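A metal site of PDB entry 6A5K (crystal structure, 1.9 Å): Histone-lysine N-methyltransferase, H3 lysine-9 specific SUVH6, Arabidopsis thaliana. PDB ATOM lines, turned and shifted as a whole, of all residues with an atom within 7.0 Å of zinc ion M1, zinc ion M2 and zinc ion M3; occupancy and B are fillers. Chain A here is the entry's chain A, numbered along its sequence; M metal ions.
The side-chain sulfur of Cys 304 sits close to the backbone NH of Cys 306 (3.4 Å).
SG of Cys 304 sits close to N of Val 307, 3.4 Å away.
The backbone NH of Cys 338 lies within hydrogen-bond range of the backbone carbonyl oxygen of Cys 292, 2.8 Å away.
The backbone carbonyl oxygen of Cys 338 is in hydrogen-bond range of the guanidinium group of Arg 345 (3.5 Å).
SG of Cys 336 lies close to N of Gly 333.
The backbone carbonyl oxygen (O) of Cys 336 lies close to the guanidinium group (NH2) of Arg 345 (3.3 Å).
O of Cys 290 sits at hydrogen-bond distance from N of Lys 337 (3.2 Å).
The backbone carbonyl oxygen (O) of Leu 344 lies within hydrogen-bond range of the backbone NH (N) of Cys 332, at 3.0 Å.
Four residues have an atom within 4 Å of zinc ion M1: Cys 290, Cys 292, Cys 296 and Cys 304.
Four residues have an atom within 4 Å of zinc ion M2: Cys 290, Cys 306, Cys 332 and Cys 336.
The nearest printed residue that does not touch zinc ion M2 is Cys 338 (4.5 Å).
The nearest printed residue that does not touch zinc ion M3 is Cys 290 (4.1 Å).
Zinc ion M1 is bound by the side-chain sulfur of Cys 296 (2.3 Å), the side-chain sulfur of Cys 304 (2.3 Å), the side-chain sulfur of Cys 292 (2.5 Å) and the side-chain sulfur of Cys 290 (2.5 Å).
Zinc ion M2 is bound by the side-chain sulfur of Cys 306 (2.3 Å), the side-chain sulfur of Cys 336 (2.3 Å), the side-chain sulfur of Cys 290 (2.4 Å) and the side-chain sulfur of Cys 332 (2.4 Å).
Zinc ion M2 has four donor atoms within binding distance.
Zinc ion M3 is bound by the side-chain sulfur of Cys 338 (2.3 Å), the side-chain sulfur of Cys 296 (2.4 Å), the side-chain sulfur of Cys 342 (2.4 Å) and the side-chain sulfur of Cys 332 (2.4 Å).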
ATOM      1  N   LYS A 288      26.817  -5.799  -9.481  1.00  0.00           N
ATOM      2  CA  LYS A 288      27.260  -5.837 -10.867  1.00  0.00           C
ATOM      3  C   LYS A 288      26.130  -5.339 -11.757  1.00  0.00           C
ATOM      4  O   LYS A 288      24.973  -5.720 -11.584  1.00  0.00           O
ATOM      5  CB  LYS A 288      27.686  -7.245 -11.274  1.00  0.00           C
ATOM      6  CG  LYS A 288      28.400  -7.313 -12.618  1.00  0.00           C
ATOM      7  CD  LYS A 288      28.210  -8.657 -13.294  1.00  0.00           C
ATOM      8  CE  LYS A 288      29.082  -8.781 -14.537  1.00  0.00           C
ATOM      9  NZ  LYS A 288      28.910  -7.626 -15.460  1.00  0.00           N
ATOM     10  N   SER A 289      26.460  -4.474 -12.723  1.00  0.00           N
ATOM     11  CA  SER A 289      25.436  -3.931 -13.608  1.00  0.00           C
ATOM     12  C   SER A 289      25.646  -4.382 -15.051  1.00  0.00           C
ATOM     13  O   SER A 289      26.707  -4.906 -15.397  1.00  0.00           O
ATOM     14  CB  SER A 289      25.419  -2.407 -13.510  1.00  0.00           C
ATOM     15  OG  SER A 289      26.707  -1.873 -13.807  1.00  0.00           O
ATOM     16  N   CYS A 290      24.629  -4.174 -15.880  1.00  0.00           N
ATOM     17  CA  CYS A 290      24.696  -4.582 -17.283  1.00  0.00           C
ATOM     18  C   CYS A 290      24.990  -3.386 -18.183  1.00  0.00           C
ATOM     19  O   CYS A 290      24.791  -2.240 -17.772  1.00  0.00           O
ATOM     20  CB  CYS A 290      23.394  -5.270 -17.717  1.00  0.00           C
ATOM     21  SG  CYS A 290      21.979  -4.162 -17.909  1.00  0.00           S
ATOM     22  N   CYS A 291      25.460  -3.646 -19.398  1.00  0.00           N
ATOM     23  CA  CYS A 291      25.857  -2.576 -20.298  1.00  0.00           C
ATOM     24  C   CYS A 291      24.849  -2.337 -21.422  1.00  0.00           C
ATOM     25  O   CYS A 291      25.136  -1.633 -22.391  1.00  0.00           O
ATOM     26  CB  CYS A 291      27.234  -2.878 -20.895  1.00  0.00           C
ATOM     27  SG  CYS A 291      27.396  -4.471 -21.719  1.00  0.00           S
ATOM     28  N   CYS A 292      23.654  -2.896 -21.278  1.00  0.00           N
ATOM     29  CA  CYS A 292      22.601  -2.755 -22.275  1.00  0.00           C
ATOM     30  C   CYS A 292      22.090  -1.325 -22.331  1.00  0.00           C
ATOM     31  O   CYS A 292      21.793  -0.724 -21.304  1.00  0.00           O
ATOM     32  CB  CYS A 292      21.448  -3.701 -21.975  1.00  0.00           C
ATOM     33  SG  CYS A 292      21.967  -5.416 -21.824  1.00  0.00           S
ATOM     34  N   THR A 293      21.976  -0.767 -23.538  1.00  0.00           N
ATOM     35  CA  THR A 293      21.474   0.591 -23.683  1.00  0.00           C
ATOM     36  C   THR A 293      19.980   0.585 -23.984  1.00  0.00           C
ATOM     37  O   THR A 293      19.288   1.575 -23.746  1.00  0.00           O
ATOM     38  CB  THR A 293      22.217   1.362 -24.804  1.00  0.00           C
ATOM     39  OG1 THR A 293      22.079   0.664 -26.047  1.00  0.00           O
ATOM     40  CG2 THR A 293      23.685   1.486 -24.469  1.00  0.00           C
ATOM     41  N   THR A 294      19.482  -0.544 -24.476  1.00  0.00           N
ATOM     42  CA  THR A 294      18.051  -0.706 -24.709  1.00  0.00           C
ATOM     43  C   THR A 294      17.462  -1.621 -23.636  1.00  0.00           C
ATOM     44  O   THR A 294      18.187  -2.092 -22.744  1.00  0.00           O
ATOM     45  CB  THR A 294      17.749  -1.300 -26.108  1.00  0.00           C
ATOM     46  OG1 THR A 294      18.163  -2.663 -26.160  1.00  0.00           O
ATOM     47  CG2 THR A 294      18.480  -0.506 -27.193  1.00  0.00           C
ATOM     48  N   ARG A 295      16.182  -1.905 -23.722  1.00  0.00           N
ATOM     49  CA  ARG A 295      15.533  -2.793 -22.765  1.00  0.00           C
ATOM     50  C   ARG A 295      16.110  -4.218 -22.851  1.00  0.00           C
ATOM     51  O   ARG A 295      16.252  -4.754 -23.912  1.00  0.00           O
ATOM     52  CB  ARG A 295      14.010  -2.718 -22.978  1.00  0.00           C
ATOM     53  CG  ARG A 295      13.364  -1.403 -22.566  1.00  0.00           C
ATOM     54  CD  ARG A 295      11.873  -1.351 -22.870  1.00  0.00           C
ATOM     55  NE  ARG A 295      11.581  -1.858 -24.194  1.00  0.00           N
ATOM     56  CZ  ARG A 295      10.400  -1.728 -24.784  1.00  0.00           C
ATOM     57  NH1 ARG A 295      10.212  -2.163 -26.010  1.00  0.00           N
ATOM     58  NH2 ARG A 295       9.409  -1.151 -24.132  1.00  0.00           N
ATOM     59  N   CYS A 296      16.390  -4.847 -21.709  1.00  0.00           N
ATOM     60  CA  CYS A 296      16.930  -6.215 -21.689  1.00  0.00           C
ATOM     61  C   CYS A 296      15.995  -7.321 -22.021  1.00  0.00           C
ATOM     62  O   CYS A 296      14.940  -7.357 -21.540  1.00  0.00           O
ATOM     63  CB  CYS A 296      17.703  -6.357 -20.329  1.00  0.00           C
ATOM     64  SG  CYS A 296      18.704  -4.932 -19.761  1.00  0.00           S
ATOM     65  N   THR A 297      16.470  -8.207 -22.859  1.00  0.00           N
ATOM     66  CA  THR A 297      15.729  -9.332 -23.397  1.00  0.00           C
ATOM     67  C   THR A 297      16.603 -10.616 -23.476  1.00  0.00           C
ATOM     68  O   THR A 297      17.767 -10.541 -23.442  1.00  0.00           O
ATOM     69  CB  THR A 297      15.113  -8.979 -24.814  1.00  0.00           C
ATOM     70  OG1 THR A 297      16.128  -8.928 -25.791  1.00  0.00           O
ATOM     71  CG2 THR A 297      14.274  -7.647 -24.900  1.00  0.00           C
ATOM     72  N   VAL A 303      25.243 -11.674 -23.382  1.00  0.00           N
ATOM     73  CA  VAL A 303      25.316 -10.231 -23.646  1.00  0.00           C
ATOM     74  C   VAL A 303      24.931  -9.421 -22.407  1.00  0.00           C
ATOM     75  O   VAL A 303      25.672  -8.525 -21.996  1.00  0.00           O
ATOM     76  CB  VAL A 303      24.411  -9.841 -24.824  1.00  0.00           C
ATOM     77  CG1 VAL A 303      24.427  -8.330 -25.034  1.00  0.00           C
ATOM     78  CG2 VAL A 303      24.846 -10.556 -26.103  1.00  0.00           C
ATOM     79  N   CYS A 304      23.784  -9.740 -21.821  1.00  0.00           N
ATOM     80  CA  CYS A 304      23.299  -9.024 -20.643  1.00  0.00           C
ATOM     81  C   CYS A 304      23.586  -9.796 -19.355  1.00  0.00           C
ATOM     82  O   CYS A 304      23.110 -10.926 -19.186  1.00  0.00           O
ATOM     83  CB  CYS A 304      21.801  -8.740 -20.745  1.00  0.00           C
ATOM     84  SG  CYS A 304      21.103  -8.010 -19.242  1.00  0.00           S
ATOM     85  N   ALA A 305      24.347  -9.179 -18.462  1.00  0.00           N
ATOM     86  CA  ALA A 305      24.729  -9.810 -17.207  1.00  0.00           C
ATOM     87  C   ALA A 305      23.513 -10.124 -16.336  1.00  0.00           C
ATOM     88  O   ALA A 305      23.484 -11.127 -15.619  1.00  0.00           O
ATOM     89  CB  ALA A 305      25.700  -8.917 -16.440  1.00  0.00           C
ATOM     90  N   CYS A 306      22.503  -9.255 -16.398  1.00  0.00           N
ATOM     91  CA  CYS A 306      21.351  -9.382 -15.523  1.00  0.00           C
ATOM     92  C   CYS A 306      20.429 -10.499 -15.999  1.00  0.00           C
ATOM     93  O   CYS A 306      19.808 -11.182 -15.188  1.00  0.00           O
ATOM     94  CB  CYS A 306      20.634  -8.042 -15.445  1.00  0.00           C
ATOM     95  SG  CYS A 306      21.733  -6.743 -14.802  1.00  0.00           S
ATOM     96  N   VAL A 307      20.336 -10.683 -17.307  1.00  0.00           N
ATOM     97  CA  VAL A 307      19.631 -11.822 -17.869  1.00  0.00           C
ATOM     98  C   VAL A 307      20.319 -13.105 -17.411  1.00  0.00           C
ATOM     99  O   VAL A 307      19.668 -14.102 -17.083  1.00  0.00           O
ATOM    100  CB  VAL A 307      19.583 -11.774 -19.408  1.00  0.00           C
ATOM    101  CG1 VAL A 307      19.065 -13.087 -19.993  1.00  0.00           C
ATOM    102  CG2 VAL A 307      18.744 -10.597 -19.869  1.00  0.00           C
ATOM    103  N   LYS A 309      22.119 -13.509 -14.656  1.00  0.00           N
ATOM    104  CA  LYS A 309      21.795 -13.726 -13.247  1.00  0.00           C
ATOM    105  C   LYS A 309      20.493 -14.514 -13.094  1.00  0.00           C
ATOM    106  O   LYS A 309      20.363 -15.363 -12.211  1.00  0.00           O
ATOM    107  CB  LYS A 309      21.660 -12.380 -12.507  1.00  0.00           C
ATOM    108  CG  LYS A 309      22.949 -11.598 -12.345  1.00  0.00           C
ATOM    109  CD  LYS A 309      22.713 -10.380 -11.445  1.00  0.00           C
ATOM    110  CE  LYS A 309      23.760  -9.294 -11.655  1.00  0.00           C
ATOM    111  NZ  LYS A 309      23.455  -8.073 -10.852  1.00  0.00           N
ATOM    112  N   GLU A 331      16.535  -7.909 -10.676  1.00  0.00           N
ATOM    113  CA  GLU A 331      16.174  -6.778 -11.513  1.00  0.00           C
ATOM    114  C   GLU A 331      17.416  -5.961 -11.832  1.00  0.00           C
ATOM    115  O   GLU A 331      18.425  -6.064 -11.134  1.00  0.00           O
ATOM    116  CB  GLU A 331      15.117  -5.910 -10.835  1.00  0.00           C
ATOM    117  CG  GLU A 331      13.778  -6.615 -10.643  1.00  0.00           C
ATOM    118  CD  GLU A 331      12.663  -5.666 -10.254  1.00  0.00           C
ATOM    119  OE1 GLU A 331      12.874  -4.430 -10.298  1.00  0.00           O
ATOM    120  OE2 GLU A 331      11.569  -6.154  -9.922  1.00  0.00           O
ATOM    121  N   CYS A 332      17.346  -5.167 -12.890  1.00  0.00           N
ATOM    122  CA  CYS A 332      18.434  -4.256 -13.200  1.00  0.00           C
ATOM    123  C   CYS A 332      18.547  -3.195 -12.114  1.00  0.00           C
ATOM    124  O   CYS A 332      17.548  -2.829 -11.488  1.00  0.00           O
ATOM    125  CB  CYS A 332      18.241  -3.636 -14.579  1.00  0.00           C
ATOM    126  SG  CYS A 332      18.579  -4.806 -15.882  1.00  0.00           S
ATOM    127  N   GLY A 333      19.766  -2.729 -11.879  1.00  0.00           N
ATOM    128  CA  GLY A 333      20.044  -1.832 -10.781  1.00  0.00           C
ATOM    129  C   GLY A 333      20.342  -0.407 -11.197  1.00  0.00           C
ATOM    130  O   GLY A 333      20.180  -0.045 -12.369  1.00  0.00           O
ATOM    131  N   LEU A 335      23.073   1.267 -11.673  1.00  0.00           N
ATOM    132  CA  LEU A 335      24.150   1.544 -12.622  1.00  0.00           C
ATOM    133  C   LEU A 335      23.993   0.808 -13.957  1.00  0.00           C
ATOM    134  O   LEU A 335      24.868   0.904 -14.820  1.00  0.00           O
ATOM    135  CB  LEU A 335      25.505   1.180 -11.999  1.00  0.00           C
ATOM    136  CG  LEU A 335      25.953   1.971 -10.769  1.00  0.00           C
ATOM    137  CD1 LEU A 335      27.457   1.851 -10.583  1.00  0.00           C
ATOM    138  CD2 LEU A 335      25.525   3.430 -10.877  1.00  0.00           C
ATOM    139  N   CYS A 336      22.891   0.072 -14.120  1.00  0.00           N
ATOM    140  CA  CYS A 336      22.597  -0.574 -15.399  1.00  0.00           C
ATOM    141  C   CYS A 336      22.302   0.496 -16.457  1.00  0.00           C
ATOM    142  O   CYS A 336      21.572   1.442 -16.193  1.00  0.00           O
ATOM    143  CB  CYS A 336      21.419  -1.535 -15.280  1.00  0.00           C
ATOM    144  SG  CYS A 336      21.758  -3.089 -14.408  1.00  0.00           S
ATOM    145  N   LYS A 337      22.873   0.338 -17.655  1.00  0.00           N
ATOM    146  CA  LYS A 337      22.764   1.362 -18.688  1.00  0.00           C
ATOM    147  C   LYS A 337      21.364   1.393 -19.319  1.00  0.00           C
ATOM    148  O   LYS A 337      21.052   2.302 -20.078  1.00  0.00           O
ATOM    149  CB  LYS A 337      23.806   1.146 -19.796  1.00  0.00           C
ATOM    150  CG  LYS A 337      25.252   1.032 -19.329  1.00  0.00           C
ATOM    151  CD  LYS A 337      26.170   0.919 -20.541  1.00  0.00           C
ATOM    152  CE  LYS A 337      27.635   1.100 -20.193  1.00  0.00           C
ATOM    153  NZ  LYS A 337      28.497   0.921 -21.409  1.00  0.00           N
ATOM    154  N   CYS A 338      20.553   0.382 -19.018  1.00  0.00           N
ATOM    155  CA  CYS A 338      19.237   0.249 -19.630  1.00  0.00           C
ATOM    156  C   CYS A 338      18.260   1.325 -19.150  1.00  0.00           C
ATOM    157  O   CYS A 338      18.421   1.875 -18.058  1.00  0.00           O
ATOM    158  CB  CYS A 338      18.676  -1.143 -19.323  1.00  0.00           C
ATOM    159  SG  CYS A 338      18.552  -1.466 -17.568  1.00  0.00           S
ATOM    160  N   PRO A 339      17.243   1.639 -19.966  1.00  0.00           N
ATOM    161  CA  PRO A 339      16.281   2.661 -19.551  1.00  0.00           C
ATOM    162  C   PRO A 339      15.371   2.199 -18.405  1.00  0.00           C
ATOM    163  O   PRO A 339      15.320   1.015 -18.064  1.00  0.00           O
ATOM    164  CB  PRO A 339      15.460   2.907 -20.823  1.00  0.00           C
ATOM    165  CG  PRO A 339      15.593   1.634 -21.600  1.00  0.00           C
ATOM    166  CD  PRO A 339      16.975   1.143 -21.329  1.00  0.00           C
ATOM    167  N   CYS A 342      12.977  -0.690 -18.779  1.00  0.00           N
ATOM    168  CA  CYS A 342      13.537  -2.029 -18.933  1.00  0.00           C
ATOM    169  C   CYS A 342      12.598  -3.089 -18.370  1.00  0.00           C
ATOM    170  O   CYS A 342      12.036  -2.916 -17.295  1.00  0.00           O
ATOM    171  CB  CYS A 342      14.893  -2.147 -18.231  1.00  0.00           C
ATOM    172  SG  CYS A 342      15.548  -3.839 -18.289  1.00  0.00           S
ATOM    173  N   TYR A 343      12.463  -4.180 -19.122  1.00  0.00           N
ATOM    174  CA  TYR A 343      11.576  -5.268 -18.713  1.00  0.00           C
ATOM    175  C   TYR A 343      11.996  -5.875 -17.371  1.00  0.00           C
ATOM    176  O   TYR A 343      11.187  -6.483 -16.667  1.00  0.00           O
ATOM    177  CB  TYR A 343      11.560  -6.344 -19.812  1.00  0.00           C
ATOM    178  CG  TYR A 343      11.026  -5.823 -21.129  1.00  0.00           C
ATOM    179  CD1 TYR A 343       9.806  -5.163 -21.196  1.00  0.00           C
ATOM    180  CD2 TYR A 343      11.754  -5.972 -22.308  1.00  0.00           C
ATOM    181  CE1 TYR A 343       9.300  -4.681 -22.395  1.00  0.00           C
ATOM    182  CE2 TYR A 343      11.257  -5.496 -23.517  1.00  0.00           C
ATOM    183  CZ  TYR A 343      10.032  -4.849 -23.549  1.00  0.00           C
ATOM    184  OH  TYR A 343       9.538  -4.385 -24.739  1.00  0.00           O
ATOM    185  N   LEU A 344      13.268  -5.682 -17.024  1.00  0.00           N
ATOM    186  CA  LEU A 344      13.791  -6.130 -15.742  1.00  0.00           C
ATOM    187  C   LEU A 344      13.762  -5.037 -14.668  1.00  0.00           C
ATOM    188  O   LEU A 344      14.499  -5.105 -13.697  1.00  0.00           O
ATOM    189  CB  LEU A 344      15.224  -6.633 -15.906  1.00  0.00           C
ATOM    190  CG  LEU A 344      15.401  -7.913 -16.713  1.00  0.00           C
ATOM    191  CD1 LEU A 344      16.884  -8.290 -16.766  1.00  0.00           C
ATOM    192  CD2 LEU A 344      14.570  -9.030 -16.100  1.00  0.00           C
ATOM    193  N   ARG A 345      12.921  -4.027 -14.855  1.00  0.00           N
ATOM    194  CA  ARG A 345      12.689  -3.048 -13.791  1.00  0.00           C
ATOM    195  C   ARG A 345      11.198  -2.990 -13.494  1.00  0.00           C
ATOM    196  O   ARG A 345      10.432  -2.378 -14.227  1.00  0.00           O
ATOM    197  CB  ARG A 345      13.211  -1.663 -14.195  1.00  0.00           C
ATOM    198  CG  ARG A 345      14.703  -1.581 -14.428  1.00  0.00           C
ATOM    199  CD  ARG A 345      15.103  -0.142 -14.741  1.00  0.00           C
ATOM    200  NE  ARG A 345      16.470  -0.008 -15.227  1.00  0.00           N
ATOM    201  CZ  ARG A 345      17.519   0.207 -14.435  1.00  0.00           C
ATOM    202  NH1 ARG A 345      17.343   0.279 -13.110  1.00  0.00           N
ATOM    203  NH2 ARG A 345      18.727   0.335 -14.953  1.00  0.00           N
HETATM  204 ZN    ZN M   1      20.867  -5.730 -19.562  1.00  0.00          ZN
HETATM  205 ZN    ZN M   2      20.987  -4.802 -15.819  1.00  0.00          ZN
HETATM  206 ZN    ZN M   3      17.915  -3.680 -17.903  1.00  0.00          ZN
